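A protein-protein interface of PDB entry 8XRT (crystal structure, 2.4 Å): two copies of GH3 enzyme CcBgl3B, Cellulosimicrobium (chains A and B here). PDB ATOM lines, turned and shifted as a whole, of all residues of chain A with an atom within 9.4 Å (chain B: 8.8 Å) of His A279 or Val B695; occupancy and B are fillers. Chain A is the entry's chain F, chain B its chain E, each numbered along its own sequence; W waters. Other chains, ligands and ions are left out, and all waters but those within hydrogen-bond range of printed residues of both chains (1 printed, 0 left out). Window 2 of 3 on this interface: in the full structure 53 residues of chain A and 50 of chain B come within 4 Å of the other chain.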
ATOM      1  N   SER A 237      -0.393  -9.569  -7.264  1.00  0.00           N
ATOM      2  CA  SER A 237      -0.890  -9.915  -8.576  1.00  0.00           C
ATOM      3  C   SER A 237      -2.132 -10.759  -8.422  1.00  0.00           C
ATOM      4  O   SER A 237      -2.317 -11.463  -7.424  1.00  0.00           O
ATOM      5  CB  SER A 237       0.158 -10.668  -9.376  1.00  0.00           C
ATOM      6  OG  SER A 237       1.160  -9.754  -9.752  1.00  0.00           O
ATOM      7  N   PRO A 242      -0.383  -8.003 -12.251  1.00  0.00           N
ATOM      8  CA  PRO A 242      -0.202  -6.983 -11.206  1.00  0.00           C
ATOM      9  C   PRO A 242      -1.398  -6.035 -11.175  1.00  0.00           C
ATOM     10  O   PRO A 242      -1.902  -5.623 -12.223  1.00  0.00           O
ATOM     11  CB  PRO A 242       1.088  -6.265 -11.636  1.00  0.00           C
ATOM     12  CG  PRO A 242       1.820  -7.297 -12.516  1.00  0.00           C
ATOM     13  CD  PRO A 242       0.738  -8.046 -13.213  1.00  0.00           C
ATOM     14  N   ASN A 270       5.090   0.459  -6.597  1.00  0.00           N
ATOM     15  CA  ASN A 270       4.393  -0.519  -7.453  1.00  0.00           C
ATOM     16  C   ASN A 270       4.882  -0.515  -8.894  1.00  0.00           C
ATOM     17  O   ASN A 270       5.023  -1.585  -9.501  1.00  0.00           O
ATOM     18  CB  ASN A 270       2.882  -0.266  -7.470  1.00  0.00           C
ATOM     19  CG  ASN A 270       2.178  -0.930  -6.300  1.00  0.00           C
ATOM     20  OD1 ASN A 270       2.829  -1.370  -5.354  1.00  0.00           O
ATOM     21  ND2 ASN A 270       0.866  -1.027  -6.368  1.00  0.00           N
ATOM     22  N   VAL A 271       5.077   0.674  -9.488  1.00  0.00           N
ATOM     23  CA  VAL A 271       5.520   0.723 -10.879  1.00  0.00           C
ATOM     24  C   VAL A 271       6.942   0.186 -11.009  1.00  0.00           C
ATOM     25  O   VAL A 271       7.241  -0.589 -11.918  1.00  0.00           O
ATOM     26  CB  VAL A 271       5.421   2.147 -11.444  1.00  0.00           C
ATOM     27  CG1 VAL A 271       6.041   2.151 -12.838  1.00  0.00           C
ATOM     28  CG2 VAL A 271       3.938   2.645 -11.466  1.00  0.00           C
ATOM     29  N   GLY A 272       7.834   0.595 -10.101  1.00  0.00           N
ATOM     30  CA  GLY A 272       9.187   0.059 -10.095  1.00  0.00           C
ATOM     31  C   GLY A 272       9.254  -1.448  -9.883  1.00  0.00           C
ATOM     32  O   GLY A 272       9.957  -2.146 -10.615  1.00  0.00           O
ATOM     33  N   ARG A 273       8.543  -1.958  -8.899  1.00  0.00           N
ATOM     34  CA  ARG A 273       8.523  -3.408  -8.621  1.00  0.00           C
ATOM     35  C   ARG A 273       8.295  -4.198  -9.903  1.00  0.00           C
ATOM     36  O   ARG A 273       8.893  -5.239 -10.048  1.00  0.00           O
ATOM     37  CB  ARG A 273       7.467  -3.699  -7.552  1.00  0.00           C
ATOM     38  CG  ARG A 273       7.896  -3.277  -6.160  1.00  0.00           C
ATOM     39  CD  ARG A 273       6.746  -3.395  -5.198  1.00  0.00           C
ATOM     40  NE  ARG A 273       6.964  -2.572  -4.031  1.00  0.00           N
ATOM     41  CZ  ARG A 273       7.616  -2.954  -2.946  1.00  0.00           C
ATOM     42  NH1 ARG A 273       8.146  -4.159  -2.870  1.00  0.00           N
ATOM     43  NH2 ARG A 273       7.747  -2.115  -1.939  1.00  0.00           N
ATOM     44  N   MET A 274       7.470  -3.697 -10.801  1.00  0.00           N
ATOM     45  CA  MET A 274       7.140  -4.453 -12.005  1.00  0.00           C
ATOM     46  C   MET A 274       8.365  -4.707 -12.877  1.00  0.00           C
ATOM     47  O   MET A 274       8.349  -5.618 -13.721  1.00  0.00           O
ATOM     48  CB  MET A 274       6.070  -3.707 -12.795  1.00  0.00           C
ATOM     49  CG  MET A 274       4.689  -3.776 -12.173  1.00  0.00           C
ATOM     50  SD  MET A 274       3.435  -3.448 -13.396  1.00  0.00           S
ATOM     51  CE  MET A 274       3.795  -1.715 -13.811  1.00  0.00           C
ATOM     52  N   VAL A 275       9.422  -3.922 -12.690  1.00  0.00           N
ATOM     53  CA  VAL A 275      10.664  -4.109 -13.422  1.00  0.00           C
ATOM     54  C   VAL A 275      11.651  -4.906 -12.570  1.00  0.00           C
ATOM     55  O   VAL A 275      12.076  -6.000 -12.953  1.00  0.00           O
ATOM     56  CB  VAL A 275      11.249  -2.746 -13.831  1.00  0.00           C
ATOM     57  CG1 VAL A 275      12.550  -2.931 -14.548  1.00  0.00           C
ATOM     58  CG2 VAL A 275      10.250  -1.979 -14.683  1.00  0.00           C
ATOM     59  N   TRP A 276      12.021  -4.371 -11.412  1.00  0.00           N
ATOM     60  CA  TRP A 276      13.154  -4.908 -10.684  1.00  0.00           C
ATOM     61  C   TRP A 276      12.804  -6.070  -9.754  1.00  0.00           C
ATOM     62  O   TRP A 276      13.717  -6.761  -9.303  1.00  0.00           O
ATOM     63  CB  TRP A 276      13.855  -3.800  -9.882  1.00  0.00           C
ATOM     64  CG  TRP A 276      13.059  -3.227  -8.742  1.00  0.00           C
ATOM     65  CD1 TRP A 276      12.375  -2.033  -8.726  1.00  0.00           C
ATOM     66  CD2 TRP A 276      12.907  -3.792  -7.423  1.00  0.00           C
ATOM     67  NE1 TRP A 276      11.801  -1.833  -7.487  1.00  0.00           N
ATOM     68  CE2 TRP A 276      12.105  -2.896  -6.673  1.00  0.00           C
ATOM     69  CE3 TRP A 276      13.378  -4.955  -6.803  1.00  0.00           C
ATOM     70  CZ2 TRP A 276      11.750  -3.144  -5.338  1.00  0.00           C
ATOM     71  CZ3 TRP A 276      13.012  -5.201  -5.477  1.00  0.00           C
ATOM     72  CH2 TRP A 276      12.205  -4.294  -4.762  1.00  0.00           C
ATOM     73  N   GLU A 277      11.526  -6.311  -9.463  1.00  0.00           N
ATOM     74  CA  GLU A 277      11.112  -7.317  -8.492  1.00  0.00           C
ATOM     75  C   GLU A 277      10.373  -8.468  -9.158  1.00  0.00           C
ATOM     76  O   GLU A 277      10.775  -9.625  -9.026  1.00  0.00           O
ATOM     77  CB  GLU A 277      10.220  -6.685  -7.406  1.00  0.00           C
ATOM     78  CG  GLU A 277      10.244  -7.428  -6.063  1.00  0.00           C
ATOM     79  CD  GLU A 277       9.117  -6.985  -5.125  1.00  0.00           C
ATOM     80  OE1 GLU A 277       8.007  -6.658  -5.619  1.00  0.00           O
ATOM     81  OE2 GLU A 277       9.347  -6.956  -3.888  1.00  0.00           O
ATOM     82  N   GLN A 278       9.314  -8.168  -9.891  1.00  0.00           N
ATOM     83  CA  GLN A 278       8.502  -9.173 -10.538  1.00  0.00           C
ATOM     84  C   GLN A 278       8.947  -9.485 -11.959  1.00  0.00           C
ATOM     85  O   GLN A 278       8.580 -10.542 -12.487  1.00  0.00           O
ATOM     86  CB  GLN A 278       7.043  -8.709 -10.533  1.00  0.00           C
ATOM     87  CG  GLN A 278       6.598  -8.249  -9.152  1.00  0.00           C
ATOM     88  CD  GLN A 278       5.382  -7.337  -9.203  1.00  0.00           C
ATOM     89  OE1 GLN A 278       5.462  -6.163  -9.621  1.00  0.00           O
ATOM     90  NE2 GLN A 278       4.243  -7.873  -8.798  1.00  0.00           N
ATOM     91  N   HIS A 279       9.713  -8.592 -12.600  1.00  0.00           N
ATOM     92  CA  HIS A 279      10.169  -8.807 -13.973  1.00  0.00           C
ATOM     93  C   HIS A 279       8.996  -9.073 -14.907  1.00  0.00           C
ATOM     94  O   HIS A 279       9.080  -9.895 -15.820  1.00  0.00           O
ATOM     95  CB  HIS A 279      11.200  -9.938 -14.038  1.00  0.00           C
ATOM     96  CG  HIS A 279      12.349  -9.735 -13.099  1.00  0.00           C
ATOM     97  ND1 HIS A 279      13.332  -8.797 -13.322  1.00  0.00           N
ATOM     98  CD2 HIS A 279      12.637 -10.300 -11.900  1.00  0.00           C
ATOM     99  CE1 HIS A 279      14.190  -8.809 -12.314  1.00  0.00           C
ATOM    100  NE2 HIS A 279      13.787  -9.707 -11.434  1.00  0.00           N
ATOM    101  N   ILE A 280       7.893  -8.370 -14.662  1.00  0.00           N
ATOM    102  CA  ILE A 280       6.712  -8.402 -15.515  1.00  0.00           C
ATOM    103  C   ILE A 280       6.841  -7.381 -16.650  1.00  0.00           C
ATOM    104  O   ILE A 280       6.216  -7.542 -17.703  1.00  0.00           O
ATOM    105  CB  ILE A 280       5.470  -8.130 -14.635  1.00  0.00           C
ATOM    106  CG1 ILE A 280       4.962  -9.366 -13.916  1.00  0.00           C
ATOM    107  CG2 ILE A 280       4.339  -7.571 -15.462  1.00  0.00           C
ATOM    108  CD1 ILE A 280       4.080 -10.258 -14.747  1.00  0.00           C
ATOM    109  N   GLN A 281       7.628  -6.312 -16.451  1.00  0.00           N
ATOM    110  CA  GLN A 281       7.849  -5.291 -17.470  1.00  0.00           C
ATOM    111  C   GLN A 281       9.338  -5.177 -17.790  1.00  0.00           C
ATOM    112  O   GLN A 281      10.171  -5.155 -16.879  1.00  0.00           O
ATOM    113  CB  GLN A 281       7.302  -3.896 -17.033  1.00  0.00           C
ATOM    114  CG  GLN A 281       5.775  -3.845 -16.878  1.00  0.00           C
ATOM    115  CD  GLN A 281       5.040  -3.831 -18.224  1.00  0.00           C
ATOM    116  OE1 GLN A 281       5.624  -3.484 -19.251  1.00  0.00           O
ATOM    117  NE2 GLN A 281       3.755  -4.217 -18.221  1.00  0.00           N
ATOM    118  N   PRO A 282       9.695  -5.074 -19.070  1.00  0.00           N
ATOM    119  CA  PRO A 282      11.126  -5.070 -19.441  1.00  0.00           C
ATOM    120  C   PRO A 282      11.895  -3.829 -19.000  1.00  0.00           C
ATOM    121  O   PRO A 282      13.110  -3.925 -18.768  1.00  0.00           O
ATOM    122  CB  PRO A 282      11.083  -5.183 -20.970  1.00  0.00           C
ATOM    123  CG  PRO A 282       9.724  -4.645 -21.351  1.00  0.00           C
ATOM    124  CD  PRO A 282       8.802  -5.038 -20.237  1.00  0.00           C
ATOM    125  N   ASP A 283      11.242  -2.674 -18.880  1.00  0.00           N
ATOM    126  CA  ASP A 283      11.929  -1.453 -18.471  1.00  0.00           C
ATOM    127  C   ASP A 283      10.923  -0.469 -17.878  1.00  0.00           C
ATOM    128  O   ASP A 283       9.715  -0.718 -17.858  1.00  0.00           O
ATOM    129  CB  ASP A 283      12.665  -0.799 -19.646  1.00  0.00           C
ATOM    130  CG  ASP A 283      11.782  -0.652 -20.868  1.00  0.00           C
ATOM    131  OD1 ASP A 283      10.675  -0.090 -20.755  1.00  0.00           O
ATOM    132  OD2 ASP A 283      12.202  -1.081 -21.956  1.00  0.00           O
ATOM    133  N   TYR A 284      11.448   0.670 -17.411  1.00  0.00           N
ATOM    134  CA  TYR A 284      10.647   1.711 -16.787  1.00  0.00           C
ATOM    135  C   TYR A 284       9.820   2.517 -17.777  1.00  0.00           C
ATOM    136  O   TYR A 284       8.827   3.124 -17.375  1.00  0.00           O
ATOM    137  CB  TYR A 284      11.541   2.663 -16.003  1.00  0.00           C
ATOM    138  CG  TYR A 284      12.040   2.073 -14.735  1.00  0.00           C
ATOM    139  CD1 TYR A 284      13.108   1.184 -14.727  1.00  0.00           C
ATOM    140  CD2 TYR A 284      11.429   2.378 -13.536  1.00  0.00           C
ATOM    141  CE1 TYR A 284      13.566   0.627 -13.534  1.00  0.00           C
ATOM    142  CE2 TYR A 284      11.871   1.829 -12.348  1.00  0.00           C
ATOM    143  CZ  TYR A 284      12.932   0.961 -12.348  1.00  0.00           C
ATOM    144  OH  TYR A 284      13.341   0.438 -11.143  1.00  0.00           O
ATOM    145  N   ALA A 287       6.746  -0.001 -17.986  1.00  0.00           N
ATOM    146  CA  ALA A 287       5.990  -0.037 -16.747  1.00  0.00           C
ATOM    147  C   ALA A 287       5.187   1.247 -16.574  1.00  0.00           C
ATOM    148  O   ALA A 287       4.022   1.211 -16.162  1.00  0.00           O
ATOM    149  CB  ALA A 287       6.945  -0.262 -15.568  1.00  0.00           C
ATOM    150  N   ARG B 624       5.727 -17.494  -8.582  1.00  0.00           N
ATOM    151  CA  ARG B 624       6.503 -16.324  -8.149  1.00  0.00           C
ATOM    152  C   ARG B 624       5.610 -15.260  -7.543  1.00  0.00           C
ATOM    153  O   ARG B 624       4.524 -14.969  -8.055  1.00  0.00           O
ATOM    154  CB  ARG B 624       7.272 -15.636  -9.298  1.00  0.00           C
ATOM    155  CG  ARG B 624       8.730 -15.982  -9.556  1.00  0.00           C
ATOM    156  CD  ARG B 624       8.893 -17.235 -10.309  1.00  0.00           C
ATOM    157  NE  ARG B 624       8.296 -17.310 -11.647  1.00  0.00           N
ATOM    158  CZ  ARG B 624       8.910 -17.048 -12.798  1.00  0.00           C
ATOM    159  NH1 ARG B 624       8.228 -17.226 -13.921  1.00  0.00           N
ATOM    160  NH2 ARG B 624      10.203 -16.697 -12.851  1.00  0.00           N
ATOM    161  N   SER B 692      12.490 -23.533 -16.168  1.00  0.00           N
ATOM    162  CA  SER B 692      12.142 -22.285 -15.513  1.00  0.00           C
ATOM    163  C   SER B 692      12.095 -21.178 -16.550  1.00  0.00           C
ATOM    164  O   SER B 692      13.094 -20.916 -17.233  1.00  0.00           O
ATOM    165  CB  SER B 692      13.142 -21.925 -14.418  1.00  0.00           C
ATOM    166  OG  SER B 692      12.807 -20.649 -13.879  1.00  0.00           O
ATOM    167  N   ASP B 693      10.945 -20.513 -16.641  1.00  0.00           N
ATOM    168  CA  ASP B 693      10.761 -19.349 -17.500  1.00  0.00           C
ATOM    169  C   ASP B 693      11.178 -18.099 -16.724  1.00  0.00           C
ATOM    170  O   ASP B 693      10.469 -17.655 -15.815  1.00  0.00           O
ATOM    171  CB  ASP B 693       9.315 -19.296 -17.967  1.00  0.00           C
ATOM    172  CG  ASP B 693       9.095 -18.265 -19.045  1.00  0.00           C
ATOM    173  OD1 ASP B 693       9.976 -17.419 -19.179  1.00  0.00           O
ATOM    174  OD2 ASP B 693       8.054 -18.284 -19.732  1.00  0.00           O
ATOM    175  N   THR B 694      12.335 -17.540 -17.079  1.00  0.00           N
ATOM    176  CA  THR B 694      13.035 -16.605 -16.191  1.00  0.00           C
ATOM    177  C   THR B 694      12.255 -15.304 -15.987  1.00  0.00           C
ATOM    178  O   THR B 694      12.146 -14.815 -14.860  1.00  0.00           O
ATOM    179  CB  THR B 694      14.444 -16.307 -16.734  1.00  0.00           C
ATOM    180  OG1 THR B 694      15.137 -17.532 -17.017  1.00  0.00           O
ATOM    181  CG2 THR B 694      15.270 -15.507 -15.708  1.00  0.00           C
ATOM    182  N   VAL B 695      11.738 -14.699 -17.050  1.00  0.00           N
ATOM    183  CA  VAL B 695      10.865 -13.540 -16.904  1.00  0.00           C
ATOM    184  C   VAL B 695       9.602 -13.832 -17.683  1.00  0.00           C
ATOM    185  O   VAL B 695       9.659 -14.335 -18.807  1.00  0.00           O
ATOM    186  CB  VAL B 695      11.494 -12.204 -17.393  1.00  0.00           C
ATOM    187  CG1 VAL B 695      12.653 -11.794 -16.518  1.00  0.00           C
ATOM    188  CG2 VAL B 695      11.927 -12.313 -18.814  1.00  0.00           C
ATOM    189  N   THR B 696       8.464 -13.521 -17.091  1.00  0.00           N
ATOM    190  CA  THR B 696       7.188 -13.838 -17.700  1.00  0.00           C
ATOM    191  C   THR B 696       6.335 -12.573 -17.729  1.00  0.00           C
ATOM    192  O   THR B 696       6.490 -11.687 -16.885  1.00  0.00           O
ATOM    193  CB  THR B 696       6.501 -14.979 -16.906  1.00  0.00           C
ATOM    194  OG1 THR B 696       6.477 -14.630 -15.512  1.00  0.00           O
ATOM    195  CG2 THR B 696       7.301 -16.265 -17.041  1.00  0.00           C
ATOM    196  N   SER B 697       5.444 -12.482 -18.717  1.00  0.00           N
ATOM    197  CA  SER B 697       4.538 -11.344 -18.802  1.00  0.00           C
ATOM    198  C   SER B 697       3.329 -11.486 -17.875  1.00  0.00           C
ATOM    199  O   SER B 697       2.533 -10.551 -17.753  1.00  0.00           O
ATOM    200  CB  SER B 697       4.062 -11.169 -20.241  1.00  0.00           C
ATOM    201  OG  SER B 697       3.166 -12.214 -20.582  1.00  0.00           O
ATOM    202  N   VAL B 698       3.161 -12.644 -17.252  1.00  0.00           N
ATOM    203  CA  VAL B 698       2.141 -12.905 -16.250  1.00  0.00           C
ATOM    204  C   VAL B 698       2.836 -13.725 -15.174  1.00  0.00           C
ATOM    205  O   VAL B 698       3.850 -14.377 -15.431  1.00  0.00           O
ATOM    206  CB  VAL B 698       0.936 -13.667 -16.831  1.00  0.00           C
ATOM    207  CG1 VAL B 698       0.176 -12.791 -17.814  1.00  0.00           C
ATOM    208  CG2 VAL B 698       1.419 -14.946 -17.509  1.00  0.00           C
ATOM    209  N   THR B 699       2.320 -13.661 -13.954  1.00  0.00           N
ATOM    210  CA  THR B 699       2.932 -14.436 -12.884  1.00  0.00           C
ATOM    211  C   THR B 699       2.796 -15.931 -13.177  1.00  0.00           C
ATOM    212  O   THR B 699       1.744 -16.403 -13.620  1.00  0.00           O
ATOM    213  CB  THR B 699       2.288 -14.104 -11.541  1.00  0.00           C
ATOM    214  OG1 THR B 699       0.895 -14.470 -11.572  1.00  0.00           O
ATOM    215  CG2 THR B 699       2.471 -12.624 -11.191  1.00  0.00           C
ATOM    216  N   TRP B 700       3.866 -16.679 -12.912  1.00  0.00           N
ATOM    217  CA  TRP B 700       3.920 -18.090 -13.273  1.00  0.00           C
ATOM    218  C   TRP B 700       4.728 -18.863 -12.234  1.00  0.00           C
ATOM    219  O   TRP B 700       5.356 -18.284 -11.337  1.00  0.00           O
ATOM    220  CB  TRP B 700       4.516 -18.269 -14.682  1.00  0.00           C
ATOM    221  CG  TRP B 700       4.254 -19.608 -15.293  1.00  0.00           C
ATOM    222  CD1 TRP B 700       5.178 -20.544 -15.648  1.00  0.00           C
ATOM    223  CD2 TRP B 700       2.985 -20.160 -15.617  1.00  0.00           C
ATOM    224  NE1 TRP B 700       4.571 -21.639 -16.184  1.00  0.00           N
ATOM    225  CE2 TRP B 700       3.219 -21.436 -16.180  1.00  0.00           C
ATOM    226  CE3 TRP B 700       1.670 -19.701 -15.499  1.00  0.00           C
ATOM    227  CZ2 TRP B 700       2.190 -22.252 -16.617  1.00  0.00           C
ATOM    228  CZ3 TRP B 700       0.657 -20.506 -15.937  1.00  0.00           C
ATOM    229  CH2 TRP B 700       0.918 -21.774 -16.481  1.00  0.00           C
ATOM    230  N   ALA B 701       4.668 -20.195 -12.350  1.00  0.00           N
ATOM    231  CA  ALA B 701       5.478 -21.080 -11.513  1.00  0.00           C
ATOM    232  C   ALA B 701       6.962 -20.788 -11.707  1.00  0.00           C
ATOM    233  O   ALA B 701       7.422 -20.585 -12.834  1.00  0.00           O
ATOM    234  CB  ALA B 701       5.195 -22.539 -11.870  1.00  0.00           C
ATOM    235  N   GLU B 702       7.713 -20.768 -10.599  1.00  0.00           N
ATOM    236  CA  GLU B 702       9.156 -20.598 -10.694  1.00  0.00           C
ATOM    237  C   GLU B 702       9.804 -21.693 -11.536  1.00  0.00           C
ATOM    238  O   GLU B 702      10.744 -21.418 -12.288  1.00  0.00           O
ATOM    239  CB  GLU B 702       9.788 -20.569  -9.301  1.00  0.00           C
ATOM    240  CG  GLU B 702      11.039 -19.660  -9.216  1.00  0.00           C
ATOM    241  CD  GLU B 702      12.286 -20.328  -9.766  1.00  0.00           C
ATOM    242  OE1 GLU B 702      12.458 -21.534  -9.500  1.00  0.00           O
ATOM    243  OE2 GLU B 702      13.100 -19.666 -10.462  1.00  0.00           O
ATOM    244  N   LEU B 732       3.312 -21.043 -20.923  1.00  0.00           N
ATOM    245  CA  LEU B 732       2.567 -20.509 -19.799  1.00  0.00           C
ATOM    246  C   LEU B 732       1.186 -20.158 -20.315  1.00  0.00           C
ATOM    247  O   LEU B 732       0.915 -20.253 -21.514  1.00  0.00           O
ATOM    248  CB  LEU B 732       3.284 -19.310 -19.149  1.00  0.00           C
ATOM    249  CG  LEU B 732       3.668 -18.135 -20.037  1.00  0.00           C
ATOM    250  CD1 LEU B 732       2.493 -17.240 -20.370  1.00  0.00           C
ATOM    251  CD2 LEU B 732       4.684 -17.349 -19.247  1.00  0.00           C
ATOM    252  N   GLU B 742       6.335 -18.228 -24.717  1.00  0.00           N
ATOM    253  CA  GLU B 742       6.662 -16.826 -24.691  1.00  0.00           C
ATOM    254  C   GLU B 742       8.166 -16.678 -24.873  1.00  0.00           C
ATOM    255  O   GLU B 742       8.920 -17.257 -24.077  1.00  0.00           O
ATOM    256  CB  GLU B 742       6.204 -16.228 -23.364  1.00  0.00           C
ATOM    257  CG  GLU B 742       6.002 -14.731 -23.373  1.00  0.00           C
ATOM    258  CD  GLU B 742       5.261 -14.215 -22.123  1.00  0.00           C
ATOM    259  OE1 GLU B 742       4.016 -14.011 -22.210  1.00  0.00           O
ATOM    260  OE2 GLU B 742       5.926 -13.984 -21.081  1.00  0.00           O
ATOM    261  N   PRO B 743       8.651 -15.940 -25.882  1.00  0.00           N
ATOM    262  CA  PRO B 743      10.098 -15.920 -26.167  1.00  0.00           C
ATOM    263  C   PRO B 743      10.922 -15.295 -25.049  1.00  0.00           C
ATOM    264  O   PRO B 743      10.425 -14.557 -24.197  1.00  0.00           O
ATOM    265  CB  PRO B 743      10.209 -15.094 -27.458  1.00  0.00           C
ATOM    266  CG  PRO B 743       8.853 -15.064 -28.034  1.00  0.00           C
ATOM    267  CD  PRO B 743       7.865 -15.231 -26.908  1.00  0.00           C
ATOM    268  N   GLY B 744      12.220 -15.606 -25.061  1.00  0.00           N
ATOM    269  CA  GLY B 744      13.113 -15.071 -24.060  1.00  0.00           C
ATOM    270  C   GLY B 744      13.952 -16.161 -23.422  1.00  0.00           C
ATOM    271  O   GLY B 744      14.106 -17.266 -23.961  1.00  0.00           O
ATOM    272  N   GLU B 745      14.518 -15.825 -22.274  1.00  0.00           N
ATOM    273  CA  GLU B 745      15.417 -16.721 -21.567  1.00  0.00           C
ATOM    274  C   GLU B 745      14.655 -17.775 -20.773  1.00  0.00           C
ATOM    275  O   GLU B 745      13.635 -17.492 -20.140  1.00  0.00           O
ATOM    276  CB  GLU B 745      16.316 -15.927 -20.628  1.00  0.00           C
ATOM    277  CG  GLU B 745      17.343 -15.043 -21.352  1.00  0.00           C
ATOM    278  CD  GLU B 745      18.469 -15.848 -22.007  1.00  0.00           C
ATOM    279  OE1 GLU B 745      19.538 -15.999 -21.364  1.00  0.00           O
ATOM    280  OE2 GLU B 745      18.293 -16.316 -23.167  1.00  0.00           O
ATOM    281  N   PHE B 746      15.172 -18.991 -20.806  1.00  0.00           N
ATOM    282  CA  PHE B 746      14.732 -20.076 -19.954  1.00  0.00           C
ATOM    283  C   PHE B 746      15.945 -20.664 -19.248  1.00  0.00           C
ATOM    284  O   PHE B 746      17.091 -20.475 -19.663  1.00  0.00           O
ATOM    285  CB  PHE B 746      14.032 -21.190 -20.744  1.00  0.00           C
ATOM    286  CG  PHE B 746      12.703 -20.795 -21.361  1.00  0.00           C
ATOM    287  CD1 PHE B 746      12.659 -20.001 -22.509  1.00  0.00           C
ATOM    288  CD2 PHE B 746      11.500 -21.280 -20.821  1.00  0.00           C
ATOM    289  CE1 PHE B 746      11.460 -19.672 -23.091  1.00  0.00           C
ATOM    290  CE2 PHE B 746      10.283 -20.975 -21.401  1.00  0.00           C
ATOM    291  CZ  PHE B 746      10.258 -20.146 -22.543  1.00  0.00           C
ATOM    292  N   GLU B 747      15.682 -21.418 -18.192  1.00  0.00           N
ATOM    293  CA  GLU B 747      16.730 -22.148 -17.498  1.00  0.00           C
ATOM    294  C   GLU B 747      16.306 -23.603 -17.431  1.00  0.00           C
ATOM    295  O   GLU B 747      15.151 -23.898 -17.109  1.00  0.00           O
ATOM    296  CB  GLU B 747      16.949 -21.561 -16.112  1.00  0.00           C
ATOM    297  CG  GLU B 747      18.312 -21.699 -15.560  1.00  0.00           C
ATOM    298  CD  GLU B 747      18.491 -20.852 -14.311  1.00  0.00           C
ATOM    299  OE1 GLU B 747      18.246 -21.368 -13.193  1.00  0.00           O
ATOM    300  OE2 GLU B 747      18.855 -19.659 -14.452  1.00  0.00           O
HETATM  301  O   HOH W   1       8.178 -12.388 -14.539  1.00  0.00           O
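O of His A279 lies close to O of Thr B696 (3.3 Å).
The backbone carbonyl oxygen of Met A274 lies within hydrogen-bond range of the backbone NH of His A279 (3.5 Å).
The backbone carbonyl oxygen (O) of Met A274 is in hydrogen-bond range of the backbone NH (N) of Ile A280.
The side-chain hydroxyl of Thr B696 is in hydrogen-bond range of the backbone carbonyl oxygen of Val B698 (2.6 Å).
The side-chain hydroxyl of Ser B697 lies within hydrogen-bond range of the side-chain carboxylate of Glu B742 (2.6 Å).
The backbone carbonyl oxygen (O) of Val A275 sits at hydrogen-bond distance from a ring nitrogen (ND1) of His A279 (3.1 Å).
Among the printed residues, pairs that only touch across the chains: Ser A237 with Thr B699 (3.5 Å), His A279 with Val B695 (3.4 Å), Ile A280 with Thr B696 (3.5 Å), Ile A280 with Ser B697 (3.4 Å), Ile A280 with Val B698 (3.6 Å) and Ile A280 with Thr B699 (3.9 Å).
Of the printed residues of chain B, Ser A237 touches Thr B699.
His A279 touches two residues of chain B.
Of the printed residues of chain B, Ile A280 touches Thr B696 (3.5 Å), Ser B697 (3.4 Å), Val B698 (3.6 Å) and Thr B699 (3.9 Å).
Thr B694 touches none of the printed residues of chain A.
Val B695 touches just one residue of chain A: His A279 (3.4 Å).
Thr B696 touches two residues of chain A.
Printed residues of chain A within 4 Å of Val B698: Ile A280.
Printed residues of chain A within 4 Å of Thr B699: Ser A237 and Ile A280.
The nearest residue of chain A that does not touch Val B695 is Gln A278 (5.8 Å).
Of the 18 printed residues of chain A, 3 touch a printed residue of chain B.
Of the 19 printed residues of chain B, 5 touch a printed residue of chain A.
Printed residues of chain B that touch a printed residue of chain A: Val B695, Thr B696, Ser B697, Val B698 and Thr B699.
Hydrophobic or aromatic side chains of chain B within 4 Å of the printed part of chain A: Val B695.
Along chain B the printed residues that touch a printed residue of chain A span positions 695 to 699.
Among the printed residues, no Asp or Glu carboxylate lies within 4 Å of a Lys or Arg side-chain nitrogen of the other chain.
No position is printed for both chains.
Of the 7 pairs that touch across the chains among the printed residues, none has its exchanged pair printed and touching as well.
Water W1 lies within hydrogen-bond range of O of Gln A278, N of Thr B696 and O of His A279.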
